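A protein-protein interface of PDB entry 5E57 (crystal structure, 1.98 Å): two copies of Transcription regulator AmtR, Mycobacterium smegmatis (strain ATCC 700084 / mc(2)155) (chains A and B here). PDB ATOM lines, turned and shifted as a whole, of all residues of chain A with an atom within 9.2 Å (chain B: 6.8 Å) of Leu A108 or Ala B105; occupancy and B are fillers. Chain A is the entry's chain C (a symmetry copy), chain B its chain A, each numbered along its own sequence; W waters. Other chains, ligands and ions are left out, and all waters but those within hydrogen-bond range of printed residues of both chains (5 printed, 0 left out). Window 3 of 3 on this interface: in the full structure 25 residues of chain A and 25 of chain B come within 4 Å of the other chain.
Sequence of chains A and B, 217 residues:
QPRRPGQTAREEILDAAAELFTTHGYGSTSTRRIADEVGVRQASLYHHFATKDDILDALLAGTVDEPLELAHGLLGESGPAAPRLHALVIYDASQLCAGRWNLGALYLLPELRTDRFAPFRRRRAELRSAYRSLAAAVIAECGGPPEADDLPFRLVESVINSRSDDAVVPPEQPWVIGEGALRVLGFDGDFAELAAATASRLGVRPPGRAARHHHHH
Among the printed residues, pairs that only touch across the chains: Arg A154 with Asn B161, Leu A108 with Ser B164, Pro A110 with Thr B22 and Leu A108 with Ala B105.
The guanidinium group of Arg A124 lies within salt-bridge range of the side-chain carboxylate of Glu A157, at 3.0 Å.
Of chain B, only Ala B105 (3.9 Å) and Ser B164 (3.6 Å) come within 4 Å of Leu A108. Of the printed residues of chain A, Thr B22 touches Pro A110. Leu B103 touches none of the printed residues of chain A. No residue of chain A comes within 4 Å of Gly B104. Ala B105 touches one residue of chain A. Of the printed residues of chain A, Asn B161 touches Arg A154. Of the printed residues of chain A, Ser B164 touches Leu A108. Printed residues of chain A within 4 Å of Asp B165: Arg A124 (2.6 Å) and Arg A154 (2.8 Å). The nearest residue of chain A that does not touch Ala B105 is Leu A109 (6.7 Å). The nearest printed residue of chain A that does not touch Asn B161 is Glu A157 (4.3 Å).
Of the 13 printed residues of chain B, 5 touch a printed residue of chain A. Printed residues of chain B that touch a printed residue of chain A: Thr B22, Ala B105, Asn B161, Ser B164 and Asp B165. Among the printed residues, 6 pairs touch across the chains.
Leu A108 touches Ala B105, but with the chains exchanged Ala A105 does not touch Leu B108 (4.1 Å).
Water W3 bridges the side-chain amide nitrogen (ND2) of Asn B161 and the side-chain amide nitrogen (ND2) of Asn A161. Water W5 lies within hydrogen-bond range of OE2 of Glu A157 (2.7 Å), NH1 of Arg A154 (2.8 Å) and OD1 of Asn B161 (3.5 Å). Water W2 lies within hydrogen-bond range of the side-chain carboxylate of Glu A157, the side-chain amide oxygen of Asn B161 and the guanidinium group of Arg A124. Water W1 bridges ND2 of Asn A161 (2.9 Å) and OD1 of Asn B161 (3.0 Å). Water W4 bridges OD1 of Asn A161 (3.0 Å) and ND2 of Asn B161 (3.1 Å).
The guanidinium group (NH1) of Arg A124 lies within salt-bridge range of the side-chain carboxylate (OD1) of Asp B165 (2.6 Å). The side-chain carboxylate (OD2) of Asp B165 lies within salt-bridge range of the guanidinium group (NH1) of Arg A154.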
ATOM      1  N   TYR A  26     -19.767  15.543  -8.334  1.00  0.00           N
ATOM      2  CA  TYR A  26     -19.947  16.811  -9.030  1.00  0.00           C
ATOM      3  C   TYR A  26     -20.909  17.716  -8.294  1.00  0.00           C
ATOM      4  O   TYR A  26     -20.516  18.789  -7.847  1.00  0.00           O
ATOM      5  CB  TYR A  26     -20.423  16.577 -10.471  1.00  0.00           C
ATOM      6  CG  TYR A  26     -20.562  17.859 -11.238  1.00  0.00           C
ATOM      7  CD1 TYR A  26     -19.429  18.541 -11.679  1.00  0.00           C
ATOM      8  CD2 TYR A  26     -21.834  18.418 -11.504  1.00  0.00           C
ATOM      9  CE1 TYR A  26     -19.558  19.761 -12.376  1.00  0.00           C
ATOM     10  CE2 TYR A  26     -21.954  19.626 -12.194  1.00  0.00           C
ATOM     11  CZ  TYR A  26     -20.816  20.281 -12.635  1.00  0.00           C
ATOM     12  OH  TYR A  26     -20.889  21.496 -13.306  1.00  0.00           O
ATOM     13  N   LEU A  56     -16.472  21.370 -15.744  1.00  0.00           N
ATOM     14  CA  LEU A  56     -16.892  20.052 -16.279  1.00  0.00           C
ATOM     15  C   LEU A  56     -16.752  19.961 -17.775  1.00  0.00           C
ATOM     16  O   LEU A  56     -16.181  18.971 -18.302  1.00  0.00           O
ATOM     17  CB  LEU A  56     -18.349  19.729 -15.860  1.00  0.00           C
ATOM     18  CG  LEU A  56     -18.823  18.301 -16.068  1.00  0.00           C
ATOM     19  CD1 LEU A  56     -17.854  17.275 -15.450  1.00  0.00           C
ATOM     20  CD2 LEU A  56     -20.207  18.135 -15.522  1.00  0.00           C
ATOM     21  N   LEU A  60     -14.568  17.185 -19.666  1.00  0.00           N
ATOM     22  CA  LEU A  60     -15.160  16.216 -20.585  1.00  0.00           C
ATOM     23  C   LEU A  60     -14.568  16.257 -22.032  1.00  0.00           C
ATOM     24  O   LEU A  60     -14.233  15.191 -22.585  1.00  0.00           O
ATOM     25  CB  LEU A  60     -16.681  16.403 -20.686  1.00  0.00           C
ATOM     26  CG  LEU A  60     -17.551  16.250 -19.417  1.00  0.00           C
ATOM     27  CD1 LEU A  60     -19.026  16.600 -19.643  1.00  0.00           C
ATOM     28  CD2 LEU A  60     -17.366  14.842 -18.912  1.00  0.00           C
ATOM     29  N   ASN A 102     -10.142   9.509 -13.218  1.00  0.00           N
ATOM     30  CA  ASN A 102     -10.933   8.618 -14.047  1.00  0.00           C
ATOM     31  C   ASN A 102     -12.133   9.423 -14.565  1.00  0.00           C
ATOM     32  O   ASN A 102     -13.268   9.185 -14.238  1.00  0.00           O
ATOM     33  CB  ASN A 102     -11.305   7.397 -13.271  1.00  0.00           C
ATOM     34  CG  ASN A 102     -12.072   6.412 -14.089  1.00  0.00           C
ATOM     35  OD1 ASN A 102     -11.909   6.340 -15.323  1.00  0.00           O
ATOM     36  ND2 ASN A 102     -12.955   5.669 -13.419  1.00  0.00           N
ATOM     37  N   LEU A 103     -11.819  10.418 -15.360  1.00  0.00           N
ATOM     38  CA  LEU A 103     -12.849  11.397 -15.780  1.00  0.00           C
ATOM     39  C   LEU A 103     -14.073  10.811 -16.497  1.00  0.00           C
ATOM     40  O   LEU A 103     -15.191  11.366 -16.480  1.00  0.00           O
ATOM     41  CB  LEU A 103     -12.214  12.435 -16.659  1.00  0.00           C
ATOM     42  CG  LEU A 103     -11.277  13.403 -15.920  1.00  0.00           C
ATOM     43  CD1 LEU A 103     -10.602  14.254 -16.987  1.00  0.00           C
ATOM     44  CD2 LEU A 103     -12.037  14.277 -14.938  1.00  0.00           C
ATOM     45  N   GLY A 104     -13.854   9.705 -17.181  1.00  0.00           N
ATOM     46  CA  GLY A 104     -14.920   9.094 -17.970  1.00  0.00           C
ATOM     47  C   GLY A 104     -16.045   8.695 -17.078  1.00  0.00           C
ATOM     48  O   GLY A 104     -17.188   8.408 -17.536  1.00  0.00           O
ATOM     49  N   ALA A 105     -15.728   8.561 -15.811  1.00  0.00           N
ATOM     50  CA  ALA A 105     -16.757   8.183 -14.836  1.00  0.00           C
ATOM     51  C   ALA A 105     -17.869   9.219 -14.743  1.00  0.00           C
ATOM     52  O   ALA A 105     -18.996   8.935 -14.370  1.00  0.00           O
ATOM     53  CB  ALA A 105     -16.134   7.987 -13.490  1.00  0.00           C
ATOM     54  N   LEU A 106     -17.570  10.429 -15.149  1.00  0.00           N
ATOM     55  CA  LEU A 106     -18.577  11.481 -15.084  1.00  0.00           C
ATOM     56  C   LEU A 106     -19.637  11.449 -16.222  1.00  0.00           C
ATOM     57  O   LEU A 106     -20.639  12.192 -16.179  1.00  0.00           O
ATOM     58  CB  LEU A 106     -17.853  12.817 -15.066  1.00  0.00           C
ATOM     59  CG  LEU A 106     -16.773  12.905 -13.958  1.00  0.00           C
ATOM     60  CD1 LEU A 106     -16.075  14.253 -14.077  1.00  0.00           C
ATOM     61  CD2 LEU A 106     -17.282  12.687 -12.524  1.00  0.00           C
ATOM     62  N   TYR A 107     -19.383  10.636 -17.247  1.00  0.00           N
ATOM     63  CA  TYR A 107     -20.286  10.518 -18.391  1.00  0.00           C
ATOM     64  C   TYR A 107     -21.691  10.224 -17.952  1.00  0.00           C
ATOM     65  O   TYR A 107     -22.609  10.627 -18.583  1.00  0.00           O
ATOM     66  CB  TYR A 107     -19.830   9.445 -19.369  1.00  0.00           C
ATOM     67  CG  TYR A 107     -18.549   9.740 -20.119  1.00  0.00           C
ATOM     68  CD1 TYR A 107     -17.963  10.989 -20.112  1.00  0.00           C
ATOM     69  CD2 TYR A 107     -17.936   8.760 -20.835  1.00  0.00           C
ATOM     70  CE1 TYR A 107     -16.784  11.241 -20.804  1.00  0.00           C
ATOM     71  CE2 TYR A 107     -16.768   8.988 -21.516  1.00  0.00           C
ATOM     72  CZ  TYR A 107     -16.181  10.252 -21.496  1.00  0.00           C
ATOM     73  OH  TYR A 107     -15.015  10.471 -22.202  1.00  0.00           O
ATOM     74  N   LEU A 108     -21.846   9.503 -16.864  1.00  0.00           N
ATOM     75  CA  LEU A 108     -23.157   9.096 -16.419  1.00  0.00           C
ATOM     76  C   LEU A 108     -23.777  10.061 -15.432  1.00  0.00           C
ATOM     77  O   LEU A 108     -24.853   9.765 -14.929  1.00  0.00           O
ATOM     78  CB  LEU A 108     -23.114   7.718 -15.767  1.00  0.00           C
ATOM     79  CG  LEU A 108     -22.532   6.583 -16.607  1.00  0.00           C
ATOM     80  CD1 LEU A 108     -22.626   5.242 -15.874  1.00  0.00           C
ATOM     81  CD2 LEU A 108     -23.183   6.558 -18.004  1.00  0.00           C
ATOM     82  N   LEU A 109     -23.125  11.190 -15.142  1.00  0.00           N
ATOM     83  CA  LEU A 109     -23.776  12.176 -14.300  1.00  0.00           C
ATOM     84  C   LEU A 109     -25.112  12.553 -14.912  1.00  0.00           C
ATOM     85  O   LEU A 109     -25.222  12.819 -16.091  1.00  0.00           O
ATOM     86  CB  LEU A 109     -22.936  13.435 -14.159  1.00  0.00           C
ATOM     87  CG  LEU A 109     -22.033  13.769 -12.957  1.00  0.00           C
ATOM     88  CD1 LEU A 109     -21.919  12.774 -11.818  1.00  0.00           C
ATOM     89  CD2 LEU A 109     -20.677  14.200 -13.430  1.00  0.00           C
ATOM     90  N   PRO A 110     -26.133  12.681 -14.093  1.00  0.00           N
ATOM     91  CA  PRO A 110     -27.416  13.135 -14.652  1.00  0.00           C
ATOM     92  C   PRO A 110     -27.361  14.575 -15.160  1.00  0.00           C
ATOM     93  O   PRO A 110     -28.060  14.944 -16.048  1.00  0.00           O
ATOM     94  CB  PRO A 110     -28.363  13.019 -13.481  1.00  0.00           C
ATOM     95  CG  PRO A 110     -27.703  12.031 -12.557  1.00  0.00           C
ATOM     96  CD  PRO A 110     -26.238  12.268 -12.687  1.00  0.00           C
ATOM     97  N   GLU A 111     -26.454  15.378 -14.652  1.00  0.00           N
ATOM     98  CA  GLU A 111     -26.256  16.733 -15.205  1.00  0.00           C
ATOM     99  C   GLU A 111     -25.937  16.789 -16.701  1.00  0.00           C
ATOM    100  O   GLU A 111     -26.249  17.786 -17.377  1.00  0.00           O
ATOM    101  CB  GLU A 111     -25.157  17.474 -14.420  1.00  0.00           C
ATOM    102  CG  GLU A 111     -25.595  17.829 -13.027  1.00  0.00           C
ATOM    103  CD  GLU A 111     -25.383  16.716 -11.995  1.00  0.00           C
ATOM    104  OE1 GLU A 111     -25.364  17.030 -10.806  1.00  0.00           O
ATOM    105  OE2 GLU A 111     -25.186  15.531 -12.340  1.00  0.00           O
ATOM    106  N   LEU A 112     -25.303  15.733 -17.214  1.00  0.00           N
ATOM    107  CA  LEU A 112     -24.959  15.684 -18.604  1.00  0.00           C
ATOM    108  C   LEU A 112     -26.187  15.459 -19.480  1.00  0.00           C
ATOM    109  O   LEU A 112     -26.092  15.647 -20.707  1.00  0.00           O
ATOM    110  CB  LEU A 112     -23.946  14.574 -18.888  1.00  0.00           C
ATOM    111  CG  LEU A 112     -22.529  15.121 -18.781  1.00  0.00           C
ATOM    112  CD1 LEU A 112     -22.306  15.748 -17.432  1.00  0.00           C
ATOM    113  CD2 LEU A 112     -21.574  13.977 -18.977  1.00  0.00           C
ATOM    114  N   ARG A 113     -27.309  15.087 -18.849  1.00  0.00           N
ATOM    115  CA  ARG A 113     -28.583  14.899 -19.590  1.00  0.00           C
ATOM    116  C   ARG A 113     -29.241  16.246 -19.991  1.00  0.00           C
ATOM    117  O   ARG A 113     -30.231  16.229 -20.691  1.00  0.00           O
ATOM    118  CB  ARG A 113     -29.574  14.077 -18.780  1.00  0.00           C
ATOM    119  CG  ARG A 113     -29.074  12.716 -18.295  1.00  0.00           C
ATOM    120  CD  ARG A 113     -30.006  12.105 -17.268  1.00  0.00           C
ATOM    121  NE  ARG A 113     -31.255  11.641 -17.896  1.00  0.00           N
ATOM    122  CZ  ARG A 113     -32.432  12.286 -17.900  1.00  0.00           C
ATOM    123  NH1 ARG A 113     -32.595  13.460 -17.287  1.00  0.00           N
ATOM    124  NH2 ARG A 113     -33.483  11.755 -18.536  1.00  0.00           N
ATOM    125  N   PHE A 120     -21.328  18.533 -25.786  1.00  0.00           N
ATOM    126  CA  PHE A 120     -20.476  17.417 -25.438  1.00  0.00           C
ATOM    127  C   PHE A 120     -21.111  16.099 -25.873  1.00  0.00           C
ATOM    128  O   PHE A 120     -20.458  15.256 -26.461  1.00  0.00           O
ATOM    129  CB  PHE A 120     -20.278  17.345 -23.961  1.00  0.00           C
ATOM    130  CG  PHE A 120     -19.596  16.113 -23.589  1.00  0.00           C
ATOM    131  CD1 PHE A 120     -18.262  15.938 -23.997  1.00  0.00           C
ATOM    132  CD2 PHE A 120     -20.275  15.096 -22.932  1.00  0.00           C
ATOM    133  CE1 PHE A 120     -17.637  14.762 -23.702  1.00  0.00           C
ATOM    134  CE2 PHE A 120     -19.666  13.919 -22.670  1.00  0.00           C
ATOM    135  CZ  PHE A 120     -18.323  13.764 -23.030  1.00  0.00           C
ATOM    136  N   ARG A 121     -22.374  15.883 -25.523  1.00  0.00           N
ATOM    137  CA  ARG A 121     -23.074  14.672 -25.946  1.00  0.00           C
ATOM    138  C   ARG A 121     -22.965  14.406 -27.418  1.00  0.00           C
ATOM    139  O   ARG A 121     -22.736  13.248 -27.841  1.00  0.00           O
ATOM    140  CB  ARG A 121     -24.536  14.703 -25.567  1.00  0.00           C
ATOM    141  CG  ARG A 121     -24.722  14.327 -24.105  1.00  0.00           C
ATOM    142  CD  ARG A 121     -26.199  14.064 -23.824  1.00  0.00           C
ATOM    143  NE  ARG A 121     -26.669  15.234 -23.140  1.00  0.00           N
ATOM    144  CZ  ARG A 121     -27.542  16.138 -23.557  1.00  0.00           C
ATOM    145  NH1 ARG A 121     -28.193  16.079 -24.713  1.00  0.00           N
ATOM    146  NH2 ARG A 121     -27.780  17.119 -22.727  1.00  0.00           N
ATOM    147  N   ARG A 124     -19.360  13.261 -28.194  1.00  0.00           N
ATOM    148  CA  ARG A 124     -19.147  11.886 -27.793  1.00  0.00           C
ATOM    149  C   ARG A 124     -19.944  10.941 -28.733  1.00  0.00           C
ATOM    150  O   ARG A 124     -19.437   9.889 -29.154  1.00  0.00           O
ATOM    151  CB  ARG A 124     -19.533  11.681 -26.316  1.00  0.00           C
ATOM    152  CG  ARG A 124     -19.376  10.245 -25.887  1.00  0.00           C
ATOM    153  CD  ARG A 124     -19.483   9.976 -24.375  1.00  0.00           C
ATOM    154  NE  ARG A 124     -19.729   8.559 -24.200  1.00  0.00           N
ATOM    155  CZ  ARG A 124     -20.946   8.027 -24.248  1.00  0.00           C
ATOM    156  NH1 ARG A 124     -22.033   8.815 -24.328  1.00  0.00           N
ATOM    157  NH2 ARG A 124     -21.098   6.721 -24.168  1.00  0.00           N
ATOM    158  N   ARG A 154     -17.838   0.214 -26.751  1.00  0.00           N
ATOM    159  CA  ARG A 154     -18.179  -0.173 -25.361  1.00  0.00           C
ATOM    160  C   ARG A 154     -16.990  -0.815 -24.640  1.00  0.00           C
ATOM    161  O   ARG A 154     -16.844  -0.628 -23.463  1.00  0.00           O
ATOM    162  CB  ARG A 154     -19.326  -1.109 -25.370  1.00  0.00           C
ATOM    163  CG  ARG A 154     -20.547  -0.560 -26.056  1.00  0.00           C
ATOM    164  CD  ARG A 154     -20.959   0.764 -25.400  1.00  0.00           C
ATOM    165  NE  ARG A 154     -22.122   1.337 -26.078  1.00  0.00           N
ATOM    166  CZ  ARG A 154     -22.660   2.486 -25.738  1.00  0.00           C
ATOM    167  NH1 ARG A 154     -22.135   3.176 -24.747  1.00  0.00           N
ATOM    168  NH2 ARG A 154     -23.709   2.962 -26.412  1.00  0.00           N
ATOM    169  N   GLU A 157     -14.675   2.077 -23.604  1.00  0.00           N
ATOM    170  CA  GLU A 157     -15.245   2.806 -22.451  1.00  0.00           C
ATOM    171  C   GLU A 157     -15.251   1.956 -21.184  1.00  0.00           C
ATOM    172  O   GLU A 157     -15.329   2.495 -20.120  1.00  0.00           O
ATOM    173  CB  GLU A 157     -16.645   3.422 -22.744  1.00  0.00           C
ATOM    174  CG  GLU A 157     -16.466   4.669 -23.638  1.00  0.00           C
ATOM    175  CD  GLU A 157     -17.594   5.618 -23.627  1.00  0.00           C
ATOM    176  OE1 GLU A 157     -17.365   6.781 -24.142  1.00  0.00           O
ATOM    177  OE2 GLU A 157     -18.642   5.212 -23.133  1.00  0.00           O
ATOM    178  N   ILE A 160     -13.118   2.633 -18.035  1.00  0.00           N
ATOM    179  CA  ILE A 160     -13.592   3.547 -17.006  1.00  0.00           C
ATOM    180  C   ILE A 160     -14.075   2.696 -15.801  1.00  0.00           C
ATOM    181  O   ILE A 160     -13.778   3.018 -14.634  1.00  0.00           O
ATOM    182  CB  ILE A 160     -14.756   4.422 -17.497  1.00  0.00           C
ATOM    183  CG1 ILE A 160     -14.283   5.369 -18.601  1.00  0.00           C
ATOM    184  CG2 ILE A 160     -15.328   5.202 -16.343  1.00  0.00           C
ATOM    185  CD1 ILE A 160     -15.351   5.883 -19.539  1.00  0.00           C
ATOM    186  N   ASN A 161     -14.805   1.614 -16.095  1.00  0.00           N
ATOM    187  CA  ASN A 161     -15.350   0.761 -15.043  1.00  0.00           C
ATOM    188  C   ASN A 161     -14.236   0.028 -14.331  1.00  0.00           C
ATOM    189  O   ASN A 161     -14.255  -0.121 -13.158  1.00  0.00           O
ATOM    190  CB  ASN A 161     -16.393  -0.209 -15.600  1.00  0.00           C
ATOM    191  CG  ASN A 161     -17.533   0.526 -16.292  1.00  0.00           C
ATOM    192  OD1 ASN A 161     -18.673   0.527 -15.827  1.00  0.00           O
ATOM    193  ND2 ASN A 161     -17.220   1.201 -17.365  1.00  0.00           N
ATOM    194  N   THR B  22     -31.374   8.281 -10.641  1.00  0.00           N
ATOM    195  CA  THR B  22     -30.753   8.091 -11.962  1.00  0.00           C
ATOM    196  C   THR B  22     -30.958   9.279 -12.887  1.00  0.00           C
ATOM    197  O   THR B  22     -30.210   9.445 -13.825  1.00  0.00           O
ATOM    198  CB  THR B  22     -31.299   6.884 -12.684  1.00  0.00           C
ATOM    199  OG1 THR B  22     -32.729   6.948 -12.659  1.00  0.00           O
ATOM    200  CG2 THR B  22     -30.817   5.622 -11.987  1.00  0.00           C
ATOM    201  N   ASN B 102     -32.204   3.026 -15.047  1.00  0.00           N
ATOM    202  CA  ASN B 102     -30.870   2.500 -15.317  1.00  0.00           C
ATOM    203  C   ASN B 102     -30.000   2.467 -14.052  1.00  0.00           C
ATOM    204  O   ASN B 102     -29.016   3.186 -13.946  1.00  0.00           O
ATOM    205  CB  ASN B 102     -30.216   3.338 -16.453  1.00  0.00           C
ATOM    206  CG  ASN B 102     -28.904   2.752 -16.950  1.00  0.00           C
ATOM    207  OD1 ASN B 102     -28.673   1.550 -16.852  1.00  0.00           O
ATOM    208  ND2 ASN B 102     -28.056   3.603 -17.529  1.00  0.00           N
ATOM    209  N   LEU B 103     -30.334   1.580 -13.113  1.00  0.00           N
ATOM    210  CA  LEU B 103     -29.691   1.595 -11.749  1.00  0.00           C
ATOM    211  C   LEU B 103     -28.211   1.312 -11.798  1.00  0.00           C
ATOM    212  O   LEU B 103     -27.467   1.782 -11.002  1.00  0.00           O
ATOM    213  CB  LEU B 103     -30.345   0.592 -10.818  1.00  0.00           C
ATOM    214  CG  LEU B 103     -31.841   0.865 -10.557  1.00  0.00           C
ATOM    215  CD1 LEU B 103     -32.513  -0.383  -9.967  1.00  0.00           C
ATOM    216  CD2 LEU B 103     -32.019   2.138  -9.720  1.00  0.00           C
ATOM    217  N   GLY B 104     -27.742   0.582 -12.801  1.00  0.00           N
ATOM    218  CA  GLY B 104     -26.320   0.299 -12.866  1.00  0.00           C
ATOM    219  C   GLY B 104     -25.510   1.536 -13.082  1.00  0.00           C
ATOM    220  O   GLY B 104     -24.279   1.538 -12.891  1.00  0.00           O
ATOM    221  N   ALA B 105     -26.175   2.603 -13.538  1.00  0.00           N
ATOM    222  CA  ALA B 105     -25.516   3.854 -13.697  1.00  0.00           C
ATOM    223  C   ALA B 105     -25.058   4.372 -12.349  1.00  0.00           C
ATOM    224  O   ALA B 105     -24.208   5.232 -12.315  1.00  0.00           O
ATOM    225  CB  ALA B 105     -26.443   4.888 -14.312  1.00  0.00           C
ATOM    226  N   LEU B 106     -25.604   3.856 -11.251  1.00  0.00           N
ATOM    227  CA  LEU B 106     -25.186   4.379  -9.924  1.00  0.00           C
ATOM    228  C   LEU B 106     -23.862   3.713  -9.394  1.00  0.00           C
ATOM    229  O   LEU B 106     -23.288   4.158  -8.402  1.00  0.00           O
ATOM    230  CB  LEU B 106     -26.339   4.164  -8.951  1.00  0.00           C
ATOM    231  CG  LEU B 106     -27.680   4.825  -9.315  1.00  0.00           C
ATOM    232  CD1 LEU B 106     -28.724   4.288  -8.349  1.00  0.00           C
ATOM    233  CD2 LEU B 106     -27.607   6.357  -9.298  1.00  0.00           C
ATOM    234  N   TYR B 107     -23.366   2.686 -10.077  1.00  0.00           N
ATOM    235  CA  TYR B 107     -22.181   1.932  -9.606  1.00  0.00           C
ATOM    236  C   TYR B 107     -20.982   2.809  -9.454  1.00  0.00           C
ATOM    237  O   TYR B 107     -20.122   2.505  -8.699  1.00  0.00           O
ATOM    238  CB  TYR B 107     -21.826   0.808 -10.578  1.00  0.00           C
ATOM    239  CG  TYR B 107     -22.805  -0.365 -10.648  1.00  0.00           C
ATOM    240  CD1 TYR B 107     -23.788  -0.566  -9.697  1.00  0.00           C
ATOM    241  CD2 TYR B 107     -22.665  -1.323 -11.618  1.00  0.00           C
ATOM    242  CE1 TYR B 107     -24.653  -1.667  -9.759  1.00  0.00           C
ATOM    243  CE2 TYR B 107     -23.503  -2.423 -11.664  1.00  0.00           C
ATOM    244  CZ  TYR B 107     -24.472  -2.583 -10.721  1.00  0.00           C
ATOM    245  OH  TYR B 107     -25.280  -3.650 -10.790  1.00  0.00           O
ATOM    246  N   LEU B 108     -20.910   3.907 -10.187  1.00  0.00           N
ATOM    247  CA  LEU B 108     -19.758   4.762 -10.161  1.00  0.00           C
ATOM    248  C   LEU B 108     -19.823   5.954  -9.178  1.00  0.00           C
ATOM    249  O   LEU B 108     -18.877   6.714  -9.056  1.00  0.00           O
ATOM    250  CB  LEU B 108     -19.564   5.297 -11.554  1.00  0.00           C
ATOM    251  CG  LEU B 108     -19.398   4.179 -12.608  1.00  0.00           C
ATOM    252  CD1 LEU B 108     -19.059   4.817 -13.973  1.00  0.00           C
ATOM    253  CD2 LEU B 108     -18.362   3.114 -12.204  1.00  0.00           C
ATOM    254  N   LEU B 109     -20.918   6.093  -8.478  1.00  0.00           N
ATOM    255  CA  LEU B 109     -21.049   7.105  -7.448  1.00  0.00           C
ATOM    256  C   LEU B 109     -19.881   6.990  -6.468  1.00  0.00           C
ATOM    257  O   LEU B 109     -19.688   5.925  -5.927  1.00  0.00           O
ATOM    258  CB  LEU B 109     -22.323   6.799  -6.719  1.00  0.00           C
ATOM    259  CG  LEU B 109     -23.613   7.599  -6.857  1.00  0.00           C
ATOM    260  CD1 LEU B 109     -23.750   8.501  -8.047  1.00  0.00           C
ATOM    261  CD2 LEU B 109     -24.820   6.675  -6.623  1.00  0.00           C
ATOM    262  N   ILE B 160     -25.423  -0.773 -19.417  1.00  0.00           N
ATOM    263  CA  ILE B 160     -25.699   0.394 -18.597  1.00  0.00           C
ATOM    264  C   ILE B 160     -25.330   1.664 -19.396  1.00  0.00           C
ATOM    265  O   ILE B 160     -26.150   2.573 -19.512  1.00  0.00           O
ATOM    266  CB  ILE B 160     -24.929   0.404 -17.290  1.00  0.00           C
ATOM    267  CG1 ILE B 160     -25.337  -0.713 -16.327  1.00  0.00           C
ATOM    268  CG2 ILE B 160     -25.111   1.752 -16.574  1.00  0.00           C
ATOM    269  CD1 ILE B 160     -24.173  -1.093 -15.385  1.00  0.00           C
ATOM    270  N   ASN B 161     -24.165   1.658 -19.996  1.00  0.00           N
ATOM    271  CA  ASN B 161     -23.759   2.744 -20.880  1.00  0.00           C
ATOM    272  C   ASN B 161     -24.669   2.860 -22.118  1.00  0.00           C
ATOM    273  O   ASN B 161     -24.976   3.959 -22.544  1.00  0.00           O
ATOM    274  CB  ASN B 161     -22.327   2.554 -21.320  1.00  0.00           C
ATOM    275  CG  ASN B 161     -21.365   2.414 -20.139  1.00  0.00           C
ATOM    276  OD1 ASN B 161     -20.606   3.329 -19.828  1.00  0.00           O
ATOM    277  ND2 ASN B 161     -21.404   1.258 -19.472  1.00  0.00           N
ATOM    278  N   SER B 164     -27.900   4.641 -21.248  1.00  0.00           N
ATOM    279  CA  SER B 164     -27.661   5.996 -21.005  1.00  0.00           C
ATOM    280  C   SER B 164     -27.619   6.758 -22.321  1.00  0.00           C
ATOM    281  O   SER B 164     -28.100   7.870 -22.385  1.00  0.00           O
ATOM    282  CB  SER B 164     -26.302   6.151 -20.357  1.00  0.00           C
ATOM    283  OG  SER B 164     -26.123   7.477 -19.941  1.00  0.00           O
ATOM    284  N   ASP B 165     -26.969   6.167 -23.311  1.00  0.00           N
ATOM    285  CA  ASP B 165     -26.834   6.801 -24.630  1.00  0.00           C
ATOM    286  C   ASP B 165     -28.151   6.743 -25.431  1.00  0.00           C
ATOM    287  O   ASP B 165     -28.473   7.689 -26.147  1.00  0.00           O
ATOM    288  CB  ASP B 165     -25.735   6.112 -25.426  1.00  0.00           C
ATOM    289  CG  ASP B 165     -24.346   6.369 -24.871  1.00  0.00           C
ATOM    290  OD1 ASP B 165     -24.221   7.331 -24.152  1.00  0.00           O
ATOM    291  OD2 ASP B 165     -23.338   5.698 -25.234  1.00  0.00           O
HETATM  292  O   HOH W   1     -18.758   3.600 -17.482  1.00  0.00           O
HETATM  293  O   HOH W   2     -20.188   6.043 -20.919  1.00  0.00           O
HETATM  294  O   HOH W   3     -18.988   0.158 -19.324  1.00  0.00           O
HETATM  295  O   HOH W   4     -21.121   2.019 -16.528  1.00  0.00           O
HETATM  296  O   HOH W   5     -19.831   2.761 -23.160  1.00  0.00           O
